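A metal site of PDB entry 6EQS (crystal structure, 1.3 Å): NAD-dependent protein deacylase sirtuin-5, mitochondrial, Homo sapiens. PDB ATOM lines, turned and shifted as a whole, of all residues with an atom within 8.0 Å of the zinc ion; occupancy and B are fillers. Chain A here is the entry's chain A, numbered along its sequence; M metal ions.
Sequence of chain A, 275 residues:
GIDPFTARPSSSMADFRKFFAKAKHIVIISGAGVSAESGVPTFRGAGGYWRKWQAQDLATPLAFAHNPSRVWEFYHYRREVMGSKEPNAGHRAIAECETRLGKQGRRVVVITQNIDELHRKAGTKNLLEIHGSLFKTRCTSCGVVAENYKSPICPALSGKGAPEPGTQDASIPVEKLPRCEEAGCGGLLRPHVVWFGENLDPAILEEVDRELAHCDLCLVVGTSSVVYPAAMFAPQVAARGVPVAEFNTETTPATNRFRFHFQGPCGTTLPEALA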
ATOM      1  N   ARG A 138     -13.388 -13.380  -8.339  1.00  0.00           N
ATOM      2  CA  ARG A 138     -14.540 -13.244  -9.285  1.00  0.00           C
ATOM      3  C   ARG A 138     -15.157 -11.851  -9.003  1.00  0.00           C
ATOM      4  O   ARG A 138     -15.290 -11.391  -7.901  1.00  0.00           O
ATOM      5  CB  ARG A 138     -15.612 -14.345  -8.859  1.00  0.00           C
ATOM      6  CG  ARG A 138     -16.775 -14.318  -9.850  1.00  0.00           C
ATOM      7  CD  ARG A 138     -17.725 -15.408  -9.869  1.00  0.00           C
ATOM      8  NE  ARG A 138     -18.412 -15.483  -8.636  1.00  0.00           N
ATOM      9  CZ  ARG A 138     -18.435 -16.477  -7.674  1.00  0.00           C
ATOM     10  NH1 ARG A 138     -17.507 -17.286  -7.594  1.00  0.00           N
ATOM     11  NH2 ARG A 138     -19.424 -16.592  -6.816  1.00  0.00           N
ATOM     12  N   CYS A 139     -15.435 -11.198 -10.115  1.00  0.00           N
ATOM     13  CA  CYS A 139     -16.057  -9.859 -10.065  1.00  0.00           C
ATOM     14  C   CYS A 139     -17.569  -9.993  -9.753  1.00  0.00           C
ATOM     15  O   CYS A 139     -18.282 -10.640 -10.500  1.00  0.00           O
ATOM     16  CB  CYS A 139     -15.831  -9.123 -11.297  1.00  0.00           C
ATOM     17  SG  CYS A 139     -16.510  -7.458 -11.282  1.00  0.00           S
ATOM     18  N   THR A 140     -17.959  -9.244  -8.691  1.00  0.00           N
ATOM     19  CA  THR A 140     -19.395  -9.273  -8.310  1.00  0.00           C
ATOM     20  C   THR A 140     -20.281  -8.451  -9.253  1.00  0.00           C
ATOM     21  O   THR A 140     -21.483  -8.502  -9.131  1.00  0.00           O
ATOM     22  CB  THR A 140     -19.567  -8.828  -6.861  1.00  0.00           C
ATOM     23  OG1 THR A 140     -19.206  -7.446  -6.716  1.00  0.00           O
ATOM     24  CG2 THR A 140     -18.852  -9.753  -5.909  1.00  0.00           C
ATOM     25  N   SER A 141     -19.675  -7.653 -10.110  1.00  0.00           N
ATOM     26  CA  SER A 141     -20.390  -6.904 -11.151  1.00  0.00           C
ATOM     27  C   SER A 141     -20.418  -7.632 -12.474  1.00  0.00           C
ATOM     28  O   SER A 141     -21.522  -7.744 -13.053  1.00  0.00           O
ATOM     29  CB  SER A 141     -19.902  -5.392 -11.253  1.00  0.00           C
ATOM     30  OG  SER A 141     -20.645  -4.828 -12.276  1.00  0.00           O
ATOM     31  N   CYS A 142     -19.236  -7.979 -13.032  1.00  0.00           N
ATOM     32  CA  CYS A 142     -19.114  -8.554 -14.367  1.00  0.00           C
ATOM     33  C   CYS A 142     -19.100 -10.098 -14.449  1.00  0.00           C
ATOM     34  O   CYS A 142     -19.275 -10.664 -15.474  1.00  0.00           O
ATOM     35  CB  CYS A 142     -18.197  -7.841 -15.381  1.00  0.00           C
ATOM     36  SG  CYS A 142     -16.510  -8.417 -14.878  1.00  0.00           S
ATOM     37  N   GLY A 143     -18.822 -10.741 -13.319  1.00  0.00           N
ATOM     38  CA  GLY A 143     -18.681 -12.162 -13.216  1.00  0.00           C
ATOM     39  C   GLY A 143     -17.342 -12.740 -13.765  1.00  0.00           C
ATOM     40  O   GLY A 143     -17.171 -13.942 -13.595  1.00  0.00           O
ATOM     41  N   VAL A 144     -16.390 -11.931 -14.106  1.00  0.00           N
ATOM     42  CA  VAL A 144     -15.218 -12.501 -14.659  1.00  0.00           C
ATOM     43  C   VAL A 144     -14.373 -13.179 -13.509  1.00  0.00           C
ATOM     44  O   VAL A 144     -14.273 -12.615 -12.426  1.00  0.00           O
ATOM     45  CB  VAL A 144     -14.335 -11.460 -15.405  1.00  0.00           C
ATOM     46  CG1 VAL A 144     -13.689 -10.451 -14.599  1.00  0.00           C
ATOM     47  CG2 VAL A 144     -13.207 -12.128 -16.167  1.00  0.00           C
ATOM     48  N   VAL A 145     -13.772 -14.292 -13.915  1.00  0.00           N
ATOM     49  CA  VAL A 145     -12.932 -15.111 -13.007  1.00  0.00           C
ATOM     50  C   VAL A 145     -11.501 -14.858 -13.427  1.00  0.00           C
ATOM     51  O   VAL A 145     -11.232 -15.017 -14.630  1.00  0.00           O
ATOM     52  CB  VAL A 145     -13.332 -16.519 -12.914  1.00  0.00           C
ATOM     53  CG1 VAL A 145     -12.247 -17.323 -12.091  1.00  0.00           C
ATOM     54  CG2 VAL A 145     -14.767 -16.712 -12.401  1.00  0.00           C
ATOM     55  N   ARG A 179     -10.637  -4.533  -6.657  1.00  0.00           N
ATOM     56  CA  ARG A 179     -11.570  -4.146  -7.712  1.00  0.00           C
ATOM     57  C   ARG A 179     -11.184  -4.705  -9.054  1.00  0.00           C
ATOM     58  O   ARG A 179     -10.031  -4.878  -9.331  1.00  0.00           O
ATOM     59  CB  ARG A 179     -11.802  -2.630  -7.786  1.00  0.00           C
ATOM     60  CG  ARG A 179     -12.608  -2.351  -6.435  1.00  0.00           C
ATOM     61  CD  ARG A 179     -12.786  -0.890  -6.332  1.00  0.00           C
ATOM     62  NE  ARG A 179     -13.593  -0.295  -7.394  1.00  0.00           N
ATOM     63  CZ  ARG A 179     -13.699   1.032  -7.651  1.00  0.00           C
ATOM     64  NH1 ARG A 179     -12.959   1.869  -7.003  1.00  0.00           N
ATOM     65  NH2 ARG A 179     -14.492   1.421  -8.559  1.00  0.00           N
ATOM     66  N   CYS A 180     -12.254  -4.935  -9.831  1.00  0.00           N
ATOM     67  CA  CYS A 180     -12.087  -5.416 -11.125  1.00  0.00           C
ATOM     68  C   CYS A 180     -11.252  -4.455 -11.999  1.00  0.00           C
ATOM     69  O   CYS A 180     -11.600  -3.314 -12.034  1.00  0.00           O
ATOM     70  CB  CYS A 180     -13.464  -5.673 -11.764  1.00  0.00           C
ATOM     71  SG  CYS A 180     -13.510  -6.531 -13.325  1.00  0.00           S
ATOM     72  N   GLU A 181     -10.350  -4.983 -12.745  1.00  0.00           N
ATOM     73  CA  GLU A 181      -9.536  -4.078 -13.646  1.00  0.00           C
ATOM     74  C   GLU A 181     -10.005  -4.123 -15.025  1.00  0.00           C
ATOM     75  O   GLU A 181      -9.408  -3.451 -15.849  1.00  0.00           O
ATOM     76  CB  GLU A 181      -8.017  -4.480 -13.540  1.00  0.00           C
ATOM     77  CG  GLU A 181      -7.427  -4.334 -12.168  1.00  0.00           C
ATOM     78  CD  GLU A 181      -5.981  -4.463 -11.970  1.00  0.00           C
ATOM     79  OE1 GLU A 181      -5.232  -5.012 -12.739  1.00  0.00           O
ATOM     80  OE2 GLU A 181      -5.555  -4.109 -10.889  1.00  0.00           O
ATOM     81  N   GLU A 182     -11.137  -4.776 -15.308  1.00  0.00           N
ATOM     82  CA  GLU A 182     -11.639  -4.714 -16.665  1.00  0.00           C
ATOM     83  C   GLU A 182     -12.117  -3.321 -16.969  1.00  0.00           C
ATOM     84  O   GLU A 182     -12.770  -2.656 -16.034  1.00  0.00           O
ATOM     85  CB  GLU A 182     -12.784  -5.690 -16.892  1.00  0.00           C
ATOM     86  CG  GLU A 182     -12.334  -7.118 -16.727  1.00  0.00           C
ATOM     87  CD  GLU A 182     -11.468  -7.689 -17.779  1.00  0.00           C
ATOM     88  OE1 GLU A 182     -11.628  -7.299 -18.922  1.00  0.00           O
ATOM     89  OE2 GLU A 182     -10.861  -8.713 -17.509  1.00  0.00           O
ATOM     90  N   ALA A 183     -11.924  -2.795 -18.182  1.00  0.00           N
ATOM     91  CA  ALA A 183     -12.220  -1.388 -18.493  1.00  0.00           C
ATOM     92  C   ALA A 183     -13.709  -1.136 -18.192  1.00  0.00           C
ATOM     93  O   ALA A 183     -14.615  -1.839 -18.674  1.00  0.00           O
ATOM     94  CB  ALA A 183     -11.919  -1.270 -19.943  1.00  0.00           C
ATOM     95  N   GLY A 184     -13.934  -0.021 -17.479  1.00  0.00           N
ATOM     96  CA  GLY A 184     -15.348   0.385 -17.214  1.00  0.00           C
ATOM     97  C   GLY A 184     -16.153  -0.504 -16.287  1.00  0.00           C
ATOM     98  O   GLY A 184     -17.344  -0.188 -16.052  1.00  0.00           O
ATOM     99  N   CYS A 185     -15.508  -1.507 -15.645  1.00  0.00           N
ATOM    100  CA  CYS A 185     -16.254  -2.327 -14.709  1.00  0.00           C
ATOM    101  C   CYS A 185     -16.020  -1.670 -13.257  1.00  0.00           C
ATOM    102  O   CYS A 185     -16.925  -1.039 -12.779  1.00  0.00           O
ATOM    103  CB  CYS A 185     -15.885  -3.757 -14.792  1.00  0.00           C
ATOM    104  SG  CYS A 185     -16.863  -4.702 -13.521  1.00  0.00           S
ATOM    105  N   GLY A 186     -14.854  -1.985 -12.725  1.00  0.00           N
ATOM    106  CA  GLY A 186     -14.511  -1.598 -11.402  1.00  0.00           C
ATOM    107  C   GLY A 186     -15.376  -2.159 -10.264  1.00  0.00           C
ATOM    108  O   GLY A 186     -15.430  -1.617  -9.115  1.00  0.00           O
ATOM    109  N   GLY A 187     -16.045  -3.251 -10.530  1.00  0.00           N
ATOM    110  CA  GLY A 187     -16.719  -3.991  -9.523  1.00  0.00           C
ATOM    111  C   GLY A 187     -15.918  -4.513  -8.364  1.00  0.00           C
ATOM    112  O   GLY A 187     -14.689  -4.713  -8.490  1.00  0.00           O
ATOM    113  N   LEU A 188     -16.546  -4.676  -7.242  1.00  0.00           N
ATOM    114  CA  LEU A 188     -15.899  -5.308  -6.117  1.00  0.00           C
ATOM    115  C   LEU A 188     -15.592  -6.809  -6.344  1.00  0.00           C
ATOM    116  O   LEU A 188     -16.508  -7.532  -6.770  1.00  0.00           O
ATOM    117  CB  LEU A 188     -16.772  -5.155  -4.880  1.00  0.00           C
ATOM    118  CG  LEU A 188     -16.279  -5.761  -3.599  1.00  0.00           C
ATOM    119  CD1 LEU A 188     -14.979  -5.151  -3.112  1.00  0.00           C
ATOM    120  CD2 LEU A 188     -17.369  -5.664  -2.571  1.00  0.00           C
ATOM    121  N   LEU A 189     -14.319  -7.157  -6.200  1.00  0.00           N
ATOM    122  CA  LEU A 189     -14.007  -8.582  -6.241  1.00  0.00           C
ATOM    123  C   LEU A 189     -14.389  -9.321  -5.019  1.00  0.00           C
ATOM    124  O   LEU A 189     -14.289  -8.752  -3.928  1.00  0.00           O
ATOM    125  CB  LEU A 189     -12.507  -8.776  -6.595  1.00  0.00           C
ATOM    126  CG  LEU A 189     -12.026  -8.038  -7.851  1.00  0.00           C
ATOM    127  CD1 LEU A 189     -10.559  -8.299  -8.091  1.00  0.00           C
ATOM    128  CD2 LEU A 189     -12.810  -8.471  -9.061  1.00  0.00           C
HETATM  129 ZN    ZN M   1     -15.803  -6.747 -13.403  1.00  0.00          ZN
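The backbone NH (N) of Cys 180 is in hydrogen-bond range of the backbone carbonyl oxygen (O) of Gly 187, at 2.8 Å. The backbone NH of Glu 182 lies close to the side-chain sulfur of Cys 180 (3.6 Å). The backbone NH (N) of Gly 187 lies close to the side-chain sulfur (SG) of Cys 185. The side-chain sulfur of Cys 142 sits close to the backbone NH of Val 144 (3.6 Å). O of Val 144 sits at hydrogen-bond distance from N of Cys 139 (2.9 Å). N of Ser 141 sits close to SG of Cys 139 (3.4 Å).
The zinc ion is bound by the side-chain sulfur of Cys 180 (2.3 Å), the side-chain sulfur of Cys 185 (2.3 Å), the side-chain sulfur of Cys 142 (2.3 Å) and the side-chain sulfur of Cys 139 (2.3 Å). The zinc ion has four donor atoms within binding distance.
Within 4 Å of the zinc ion: Cys 139, Cys 142, Cys 180 and Cys 185.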
